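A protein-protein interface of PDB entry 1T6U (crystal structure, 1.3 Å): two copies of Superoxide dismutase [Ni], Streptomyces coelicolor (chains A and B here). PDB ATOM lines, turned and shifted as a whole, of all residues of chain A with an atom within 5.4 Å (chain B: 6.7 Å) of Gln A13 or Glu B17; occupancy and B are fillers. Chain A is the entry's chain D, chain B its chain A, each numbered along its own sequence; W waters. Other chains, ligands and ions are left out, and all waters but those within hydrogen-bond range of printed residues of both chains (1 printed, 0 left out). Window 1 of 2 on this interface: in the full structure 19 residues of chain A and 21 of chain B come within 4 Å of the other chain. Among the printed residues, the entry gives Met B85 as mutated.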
ATOM      1  N   HIS A   1      24.929   4.748  -4.525  1.00  0.00           N
ATOM      2  CA  HIS A   1      25.896   3.671  -4.396  1.00  0.00           C
ATOM      3  C   HIS A   1      25.301   2.368  -4.906  1.00  0.00           C
ATOM      4  O   HIS A   1      25.955   1.325  -4.850  1.00  0.00           O
ATOM      5  CB  HIS A   1      26.363   3.475  -2.953  1.00  0.00           C
ATOM      6  CG  HIS A   1      25.202   3.455  -1.996  1.00  0.00           C
ATOM      7  ND1 HIS A   1      24.950   4.509  -1.165  1.00  0.00           N
ATOM      8  CD2 HIS A   1      24.248   2.548  -1.700  1.00  0.00           C
ATOM      9  CE1 HIS A   1      23.892   4.248  -0.417  1.00  0.00           C
ATOM     10  NE2 HIS A   1      23.430   3.052  -0.730  1.00  0.00           N
ATOM     11  N   ASP A  10      28.977   7.609   0.506  1.00  0.00           N
ATOM     12  CA  ASP A  10      29.717   8.054   1.689  1.00  0.00           C
ATOM     13  C   ASP A  10      30.748   6.999   2.022  1.00  0.00           C
ATOM     14  O   ASP A  10      30.327   5.864   2.285  1.00  0.00           O
ATOM     15  CB  ASP A  10      28.780   8.280   2.874  1.00  0.00           C
ATOM     16  CG  ASP A  10      29.442   9.040   4.001  1.00  0.00           C
ATOM     17  OD1 ASP A  10      30.681   8.933   4.148  1.00  0.00           O
ATOM     18  OD2 ASP A  10      28.691   9.775   4.697  1.00  0.00           O
ATOM     19  N   PRO A  11      32.025   7.364   2.031  1.00  0.00           N
ATOM     20  CA  PRO A  11      33.045   6.415   2.486  1.00  0.00           C
ATOM     21  C   PRO A  11      32.783   5.857   3.885  1.00  0.00           C
ATOM     22  O   PRO A  11      33.398   4.840   4.253  1.00  0.00           O
ATOM     23  CB  PRO A  11      34.339   7.243   2.464  1.00  0.00           C
ATOM     24  CG  PRO A  11      34.042   8.266   1.390  1.00  0.00           C
ATOM     25  CD  PRO A  11      32.624   8.663   1.629  1.00  0.00           C
ATOM     26  N   ALA A  12      31.867   6.477   4.614  1.00  0.00           N
ATOM     27  CA  ALA A  12      31.487   5.916   5.898  1.00  0.00           C
ATOM     28  C   ALA A  12      31.015   4.458   5.831  1.00  0.00           C
ATOM     29  O   ALA A  12      31.154   3.698   6.807  1.00  0.00           O
ATOM     30  CB  ALA A  12      30.397   6.782   6.489  1.00  0.00           C
ATOM     31  N   GLN A  13      30.433   4.040   4.711  1.00  0.00           N
ATOM     32  CA  GLN A  13      30.001   2.650   4.595  1.00  0.00           C
ATOM     33  C   GLN A  13      31.203   1.725   4.665  1.00  0.00           C
ATOM     34  O   GLN A  13      31.267   0.788   5.456  1.00  0.00           O
ATOM     35  CB  GLN A  13      29.180   2.391   3.342  1.00  0.00           C
ATOM     36  CG  GLN A  13      27.920   3.251   3.209  1.00  0.00           C
ATOM     37  CD  GLN A  13      27.047   2.774   2.062  1.00  0.00           C
ATOM     38  OE1 GLN A  13      27.304   2.957   0.872  1.00  0.00           O
ATOM     39  NE2 GLN A  13      25.931   2.122   2.420  1.00  0.00           N
ATOM     40  N   ALA A  14      32.212   1.968   3.868  1.00  0.00           N
ATOM     41  CA  ALA A  14      33.444   1.204   3.935  1.00  0.00           C
ATOM     42  C   ALA A  14      34.093   1.322   5.310  1.00  0.00           C
ATOM     43  O   ALA A  14      34.560   0.318   5.865  1.00  0.00           O
ATOM     44  CB  ALA A  14      34.441   1.681   2.873  1.00  0.00           C
ATOM     45  N   ARG A  15      34.156   2.518   5.880  1.00  0.00           N
ATOM     46  CA  ARG A  15      34.817   2.776   7.146  1.00  0.00           C
ATOM     47  C   ARG A  15      34.152   2.008   8.261  1.00  0.00           C
ATOM     48  O   ARG A  15      34.864   1.375   9.049  1.00  0.00           O
ATOM     49  CB  ARG A  15      34.831   4.263   7.450  1.00  0.00           C
ATOM     50  CG  ARG A  15      35.506   4.532   8.785  1.00  0.00           C
ATOM     51  CD  ARG A  15      35.739   6.026   8.968  1.00  0.00           C
ATOM     52  NE  ARG A  15      34.648   6.894   8.624  1.00  0.00           N
ATOM     53  CZ  ARG A  15      34.464   7.695   7.587  1.00  0.00           C
ATOM     54  NH1 ARG A  15      35.296   7.876   6.585  1.00  0.00           N
ATOM     55  NH2 ARG A  15      33.338   8.385   7.532  1.00  0.00           N
ATOM     56  N   ILE A  16      32.850   2.024   8.397  1.00  0.00           N
ATOM     57  CA  ILE A  16      32.269   1.305   9.534  1.00  0.00           C
ATOM     58  C   ILE A  16      32.522  -0.208   9.432  1.00  0.00           C
ATOM     59  O   ILE A  16      32.738  -0.861  10.453  1.00  0.00           O
ATOM     60  CB  ILE A  16      30.757   1.589   9.664  1.00  0.00           C
ATOM     61  CG1 ILE A  16      30.131   1.120  10.982  1.00  0.00           C
ATOM     62  CG2 ILE A  16      29.962   0.970   8.527  1.00  0.00           C
ATOM     63  CD1 ILE A  16      29.035   1.969  11.578  1.00  0.00           C
ATOM     64  N   GLU A  17      32.477  -0.789   8.221  1.00  0.00           N
ATOM     65  CA  GLU A  17      32.793  -2.207   8.092  1.00  0.00           C
ATOM     66  C   GLU A  17      34.253  -2.453   8.441  1.00  0.00           C
ATOM     67  O   GLU A  17      34.551  -3.448   9.120  1.00  0.00           O
ATOM     68  CB  GLU A  17      32.414  -2.708   6.713  1.00  0.00           C
ATOM     69  CG  GLU A  17      30.921  -2.647   6.417  1.00  0.00           C
ATOM     70  CD  GLU A  17      30.044  -3.424   7.374  1.00  0.00           C
ATOM     71  OE1 GLU A  17      28.791  -3.215   7.354  1.00  0.00           O
ATOM     72  OE2 GLU A  17      30.572  -4.252   8.158  1.00  0.00           O
ATOM     73  N   ALA A  18      35.154  -1.568   8.015  1.00  0.00           N
ATOM     74  CA  ALA A  18      36.563  -1.732   8.386  1.00  0.00           C
ATOM     75  C   ALA A  18      36.809  -1.570   9.879  1.00  0.00           C
ATOM     76  O   ALA A  18      37.667  -2.233  10.467  1.00  0.00           O
ATOM     77  CB  ALA A  18      37.403  -0.780   7.543  1.00  0.00           C
ATOM     78  N   HIS A  54      32.216  -1.806  -0.843  1.00  0.00           N
ATOM     79  CA  HIS A  54      32.001  -0.376  -0.701  1.00  0.00           C
ATOM     80  C   HIS A  54      33.126   0.412  -1.354  1.00  0.00           C
ATOM     81  O   HIS A  54      32.882   1.414  -2.030  1.00  0.00           O
ATOM     82  CB  HIS A  54      31.823   0.029   0.762  1.00  0.00           C
ATOM     83  CG  HIS A  54      30.602  -0.511   1.419  1.00  0.00           C
ATOM     84  ND1 HIS A  54      29.383  -0.528   0.805  1.00  0.00           N
ATOM     85  CD2 HIS A  54      30.418  -1.057   2.648  1.00  0.00           C
ATOM     86  CE1 HIS A  54      28.501  -1.074   1.654  1.00  0.00           C
ATOM     87  NE2 HIS A  54      29.108  -1.394   2.775  1.00  0.00           N
ATOM     88  N   ALA B  12      23.822   5.616  11.153  1.00  0.00           N
ATOM     89  CA  ALA B  12      24.176   6.032   9.815  1.00  0.00           C
ATOM     90  C   ALA B  12      24.045   4.947   8.773  1.00  0.00           C
ATOM     91  O   ALA B  12      23.793   5.230   7.611  1.00  0.00           O
ATOM     92  CB  ALA B  12      25.640   6.427   9.786  1.00  0.00           C
ATOM     93  N   GLN B  13      24.203   3.662   9.104  1.00  0.00           N
ATOM     94  CA  GLN B  13      24.034   2.596   8.126  1.00  0.00           C
ATOM     95  C   GLN B  13      22.599   2.598   7.612  1.00  0.00           C
ATOM     96  O   GLN B  13      22.398   2.564   6.399  1.00  0.00           O
ATOM     97  CB  GLN B  13      24.416   1.211   8.689  1.00  0.00           C
ATOM     98  CG  GLN B  13      25.843   1.104   9.203  1.00  0.00           C
ATOM     99  CD  GLN B  13      26.229  -0.343   9.444  1.00  0.00           C
ATOM    100  OE1 GLN B  13      25.884  -0.965  10.480  1.00  0.00           O
ATOM    101  NE2 GLN B  13      26.971  -0.917   8.502  1.00  0.00           N
ATOM    102  N   ALA B  14      21.644   2.662   8.548  1.00  0.00           N
ATOM    103  CA  ALA B  14      20.247   2.777   8.169  1.00  0.00           C
ATOM    104  C   ALA B  14      19.974   4.093   7.454  1.00  0.00           C
ATOM    105  O   ALA B  14      19.267   4.129   6.417  1.00  0.00           O
ATOM    106  CB  ALA B  14      19.352   2.693   9.404  1.00  0.00           C
ATOM    107  N   ARG B  15      20.502   5.214   7.975  1.00  0.00           N
ATOM    108  CA  ARG B  15      20.253   6.505   7.380  1.00  0.00           C
ATOM    109  C   ARG B  15      20.694   6.604   5.916  1.00  0.00           C
ATOM    110  O   ARG B  15      19.951   7.109   5.062  1.00  0.00           O
ATOM    111  CB  ARG B  15      20.988   7.617   8.178  1.00  0.00           C
ATOM    112  CG  ARG B  15      20.590   9.012   7.666  1.00  0.00           C
ATOM    113  CD  ARG B  15      21.360  10.099   8.363  1.00  0.00           C
ATOM    114  NE  ARG B  15      22.730  10.058   7.828  1.00  0.00           N
ATOM    115  CZ  ARG B  15      23.805   9.841   8.570  1.00  0.00           C
ATOM    116  NH1 ARG B  15      23.725   9.651   9.887  1.00  0.00           N
ATOM    117  NH2 ARG B  15      24.955   9.833   7.904  1.00  0.00           N
ATOM    118  N   ILE B  16      21.906   6.101   5.627  1.00  0.00           N
ATOM    119  CA  ILE B  16      22.363   6.286   4.250  1.00  0.00           C
ATOM    120  C   ILE B  16      21.527   5.459   3.306  1.00  0.00           C
ATOM    121  O   ILE B  16      21.254   5.925   2.201  1.00  0.00           O
ATOM    122  CB  ILE B  16      23.869   5.924   4.194  1.00  0.00           C
ATOM    123  CG1 ILE B  16      24.746   6.819   5.076  1.00  0.00           C
ATOM    124  CG2 ILE B  16      24.342   5.866   2.751  1.00  0.00           C
ATOM    125  CD1 ILE B  16      26.096   6.289   5.530  1.00  0.00           C
ATOM    126  N   GLU B  17      21.057   4.281   3.708  1.00  0.00           N
ATOM    127  CA  GLU B  17      20.188   3.497   2.800  1.00  0.00           C
ATOM    128  C   GLU B  17      18.857   4.212   2.645  1.00  0.00           C
ATOM    129  O   GLU B  17      18.347   4.250   1.523  1.00  0.00           O
ATOM    130  CB  GLU B  17      20.026   2.056   3.271  1.00  0.00           C
ATOM    131  CG  GLU B  17      21.315   1.253   3.296  1.00  0.00           C
ATOM    132  CD  GLU B  17      21.947   1.126   1.924  1.00  0.00           C
ATOM    133  OE1 GLU B  17      23.074   0.628   1.860  1.00  0.00           O
ATOM    134  OE2 GLU B  17      21.302   1.523   0.914  1.00  0.00           O
ATOM    135  N   ALA B  18      18.292   4.785   3.726  1.00  0.00           N
ATOM    136  CA  ALA B  18      17.046   5.529   3.591  1.00  0.00           C
ATOM    137  C   ALA B  18      17.234   6.773   2.750  1.00  0.00           C
ATOM    138  O   ALA B  18      16.329   7.176   2.003  1.00  0.00           O
ATOM    139  CB  ALA B  18      16.500   5.758   4.996  1.00  0.00           C
ATOM    140  N   GLU B  19      18.386   7.436   2.817  1.00  0.00           N
ATOM    141  CA  GLU B  19      18.690   8.550   1.939  1.00  0.00           C
ATOM    142  C   GLU B  19      18.668   8.119   0.468  1.00  0.00           C
ATOM    143  O   GLU B  19      18.168   8.789  -0.417  1.00  0.00           O
ATOM    144  CB  GLU B  19      20.054   9.138   2.356  1.00  0.00           C
ATOM    145  CG  GLU B  19      20.049   9.943   3.635  1.00  0.00           C
ATOM    146  CD  GLU B  19      21.420  10.400   4.078  1.00  0.00           C
ATOM    147  OE1 GLU B  19      21.510  11.046   5.155  1.00  0.00           O
ATOM    148  OE2 GLU B  19      22.428  10.117   3.391  1.00  0.00           O
ATOM    149  N   SER B  20      19.261   6.938   0.193  1.00  0.00           N
ATOM    150  CA  SER B  20      19.242   6.465  -1.185  1.00  0.00           C
ATOM    151  C   SER B  20      17.800   6.141  -1.606  1.00  0.00           C
ATOM    152  O   SER B  20      17.421   6.466  -2.732  1.00  0.00           O
ATOM    153  CB  SER B  20      20.313   5.368  -1.400  1.00  0.00           C
ATOM    154  OG  SER B  20      19.728   4.201  -0.996  1.00  0.00           O
ATOM    155  N   VAL B  21      16.955   5.574  -0.734  1.00  0.00           N
ATOM    156  CA  VAL B  21      15.565   5.367  -1.083  1.00  0.00           C
ATOM    157  C   VAL B  21      14.903   6.691  -1.502  1.00  0.00           C
ATOM    158  O   VAL B  21      14.239   6.766  -2.544  1.00  0.00           O
ATOM    159  CB  VAL B  21      14.837   4.694   0.076  1.00  0.00           C
ATOM    160  CG1 VAL B  21      13.334   4.663  -0.097  1.00  0.00           C
ATOM    161  CG2 VAL B  21      15.275   3.242   0.247  1.00  0.00           C
ATOM    162  N   LYS B  22      15.041   7.731  -0.679  1.00  0.00           N
ATOM    163  CA  LYS B  22      14.419   9.001  -1.005  1.00  0.00           C
ATOM    164  C   LYS B  22      14.937   9.586  -2.310  1.00  0.00           C
ATOM    165  O   LYS B  22      14.193  10.126  -3.129  1.00  0.00           O
ATOM    166  CB  LYS B  22      14.670  10.023   0.113  1.00  0.00           C
ATOM    167  CG  LYS B  22      13.919  11.314  -0.132  1.00  0.00           C
ATOM    168  CD  LYS B  22      14.144  12.371   0.960  1.00  0.00           C
ATOM    169  CE  LYS B  22      13.401  13.623   0.528  1.00  0.00           C
ATOM    170  NZ  LYS B  22      13.774  14.875   1.240  1.00  0.00           N
ATOM    171  N   GLN B  46      15.594  -2.966  -2.795  1.00  0.00           N
ATOM    172  CA  GLN B  46      16.804  -3.494  -2.163  1.00  0.00           C
ATOM    173  C   GLN B  46      17.334  -2.588  -1.073  1.00  0.00           C
ATOM    174  O   GLN B  46      17.692  -3.063   0.007  1.00  0.00           O
ATOM    175  CB  GLN B  46      17.881  -3.690  -3.242  1.00  0.00           C
ATOM    176  CG  GLN B  46      17.600  -4.775  -4.251  1.00  0.00           C
ATOM    177  CD  GLN B  46      18.453  -4.795  -5.489  1.00  0.00           C
ATOM    178  OE1 GLN B  46      19.076  -3.814  -5.890  1.00  0.00           O
ATOM    179  NE2 GLN B  46      18.516  -5.881  -6.243  1.00  0.00           N
ATOM    180  N   ARG B  47      17.422  -1.285  -1.350  1.00  0.00           N
ATOM    181  CA  ARG B  47      18.020  -0.419  -0.335  1.00  0.00           C
ATOM    182  C   ARG B  47      17.116  -0.299   0.883  1.00  0.00           C
ATOM    183  O   ARG B  47      17.602  -0.260   2.008  1.00  0.00           O
ATOM    184  CB  ARG B  47      18.375   0.944  -0.936  1.00  0.00           C
ATOM    185  CG  ARG B  47      19.155   0.955  -2.210  1.00  0.00           C
ATOM    186  CD  ARG B  47      20.193  -0.123  -2.412  1.00  0.00           C
ATOM    187  NE  ARG B  47      21.335  -0.052  -1.519  1.00  0.00           N
ATOM    188  CZ  ARG B  47      22.479  -0.699  -1.700  1.00  0.00           C
ATOM    189  NH1 ARG B  47      22.685  -1.490  -2.747  1.00  0.00           N
ATOM    190  NH2 ARG B  47      23.474  -0.566  -0.822  1.00  0.00           N
ATOM    191  N   ALA B  48      15.794  -0.274   0.636  1.00  0.00           N
ATOM    192  CA  ALA B  48      14.825  -0.194   1.730  1.00  0.00           C
ATOM    193  C   ALA B  48      14.946  -1.435   2.613  1.00  0.00           C
ATOM    194  O   ALA B  48      14.896  -1.348   3.836  1.00  0.00           O
ATOM    195  CB  ALA B  48      13.435  -0.036   1.191  1.00  0.00           C
ATOM    196  N   LEU B  50      17.632  -3.252   3.079  1.00  0.00           N
ATOM    197  CA  LEU B  50      18.857  -3.104   3.842  1.00  0.00           C
ATOM    198  C   LEU B  50      18.633  -2.154   5.034  1.00  0.00           C
ATOM    199  O   LEU B  50      19.093  -2.395   6.164  1.00  0.00           O
ATOM    200  CB  LEU B  50      19.968  -2.579   2.958  1.00  0.00           C
ATOM    201  CG  LEU B  50      20.599  -3.559   2.001  1.00  0.00           C
ATOM    202  CD1 LEU B  50      21.510  -2.855   1.021  1.00  0.00           C
ATOM    203  CD2 LEU B  50      21.381  -4.629   2.793  1.00  0.00           C
ATOM    204  N   ALA B  51      17.919  -1.062   4.796  1.00  0.00           N
ATOM    205  CA  ALA B  51      17.602  -0.120   5.878  1.00  0.00           C
ATOM    206  C   ALA B  51      16.814  -0.808   6.978  1.00  0.00           C
ATOM    207  O   ALA B  51      17.065  -0.590   8.165  1.00  0.00           O
ATOM    208  CB  ALA B  51      16.848   1.092   5.351  1.00  0.00           C
ATOM    209  N   LYS B  52      15.853  -1.664   6.616  1.00  0.00           N
ATOM    210  CA  LYS B  52      15.112  -2.406   7.617  1.00  0.00           C
ATOM    211  C   LYS B  52      16.018  -3.309   8.447  1.00  0.00           C
ATOM    212  O   LYS B  52      15.887  -3.368   9.687  1.00  0.00           O
ATOM    213  CB  LYS B  52      14.009  -3.220   6.953  1.00  0.00           C
ATOM    214  CG  LYS B  52      12.832  -2.406   6.430  1.00  0.00           C
ATOM    215  CD  LYS B  52      11.751  -3.285   5.804  1.00  0.00           C
ATOM    216  CE  LYS B  52      10.767  -3.811   6.810  1.00  0.00           C
ATOM    217  NZ  LYS B  52       9.901  -4.882   6.214  1.00  0.00           N
ATOM    218  N   HIS B  54      19.236  -2.866   9.094  1.00  0.00           N
ATOM    219  CA  HIS B  54      20.029  -2.053  10.000  1.00  0.00           C
ATOM    220  C   HIS B  54      19.194  -1.586  11.203  1.00  0.00           C
ATOM    221  O   HIS B  54      19.672  -1.586  12.325  1.00  0.00           O
ATOM    222  CB  HIS B  54      20.639  -0.873   9.246  1.00  0.00           C
ATOM    223  CG  HIS B  54      21.614  -1.258   8.203  1.00  0.00           C
ATOM    224  ND1 HIS B  54      22.659  -2.121   8.445  1.00  0.00           N
ATOM    225  CD2 HIS B  54      21.694  -0.847   6.930  1.00  0.00           C
ATOM    226  CE1 HIS B  54      23.338  -2.224   7.313  1.00  0.00           C
ATOM    227  NE2 HIS B  54      22.777  -1.471   6.360  1.00  0.00           N
ATOM    228  N   MET B  85       9.430   2.157   6.441  1.00  0.00           N
ATOM    229  CA  MET B  85      10.291   1.668   5.372  1.00  0.00           C
ATOM    230  C   MET B  85       9.507   0.799   4.395  1.00  0.00           C
ATOM    231  O   MET B  85       9.707   0.853   3.185  1.00  0.00           O
ATOM    232  CB  MET B  85      11.495   0.909   5.938  1.00  0.00           C
ATOM    233  CG  MET B  85      12.565   1.748   6.574  1.00  0.00           C
ATOM    234  SD  MET B  85      13.452   2.916   5.541  1.00  0.00           S
ATOM    235  CE  MET B  85      13.106   2.496   3.834  1.00  0.00           C
ATOM    236  N   LEU B 101      13.182   8.593   7.074  1.00  0.00           N
ATOM    237  CA  LEU B 101      14.334   9.336   7.613  1.00  0.00           C
ATOM    238  C   LEU B 101      14.035  10.037   8.911  1.00  0.00           C
ATOM    239  O   LEU B 101      14.883  10.089   9.830  1.00  0.00           O
ATOM    240  CB  LEU B 101      14.826  10.367   6.571  1.00  0.00           C
ATOM    241  CG  LEU B 101      15.639   9.726   5.418  1.00  0.00           C
ATOM    242  CD1 LEU B 101      15.698  10.690   4.244  1.00  0.00           C
ATOM    243  CD2 LEU B 101      17.028   9.292   5.873  1.00  0.00           C
ATOM    244  N   ILE B 104      14.083   7.390  11.531  1.00  0.00           N
ATOM    245  CA  ILE B 104      15.469   7.032  11.837  1.00  0.00           C
ATOM    246  C   ILE B 104      16.149   8.106  12.669  1.00  0.00           C
ATOM    247  O   ILE B 104      16.965   7.818  13.553  1.00  0.00           O
ATOM    248  CB  ILE B 104      16.251   6.738  10.533  1.00  0.00           C
ATOM    249  CG1 ILE B 104      15.731   5.466   9.864  1.00  0.00           C
ATOM    250  CG2 ILE B 104      17.744   6.675  10.790  1.00  0.00           C
ATOM    251  CD1 ILE B 104      16.097   5.283   8.401  1.00  0.00           C
HETATM  252  O   HOH W   1      24.815   1.344   5.118  1.00  0.00           O
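NE2 of Gln A13 lies within hydrogen-bond range of OE1 of Glu B17. OE1 of Glu A17 is in hydrogen-bond range of NE2 of Gln B13 (3.1 Å). A ring nitrogen (NE2) of His A1 is in hydrogen-bond range of the side-chain carboxylate of Glu B17, at 3.1 Å.
Water W1 bridges O of Gln B13 (3.0 Å) and NE2 of Gln A13 (3.0 Å).
Of the 21 printed residues of chain B, 5 touch a printed residue of chain A. Hydrophobic or aromatic side chains of chain B that line the printed part of chain A: Ile B16. Of the 11 printed residues of chain A, 4 touch a printed residue of chain B.
OE1 of Gln A13 is in hydrogen-bond range of ND1 of His A1, at 3.5 Å. The side-chain hydroxyl of Ser B20 lies within hydrogen-bond range of the backbone carbonyl oxygen of Glu B17 (2.9 Å). OE2 of Glu B17 lies within salt-bridge range of NE of Arg B47, 2.9 Å away.
Printed residues of chain A within 4 Å of Glu B17: His A1 and Gln A13. Printed residues of chain A within 4 Å of Ser B20: His A1 (3.9 Å). Printed residues of chain A within 4 Å of Arg B47: His A1 (3.3 Å). The nearest printed residue of chain B that does not touch Ile A16 is Ala B12 (5.9 Å).
Gln A13 touches Glu B17, and with the chains exchanged Glu A17 touches Gln B13. Ile A16 touches Gln B13, but with the chains exchanged Gln A13 does not touch Ile B16 (4.1 Å). Of the 7 pairs that touch across the chains among the printed residues, 2 have their exchanged pair printed and touching as well.
Among the printed residues, pairs that only touch across the chains: His A1 with Arg B47, Ile A16 with Gln B13, His A1 with Ile B16 and His A1 with Ser B20.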
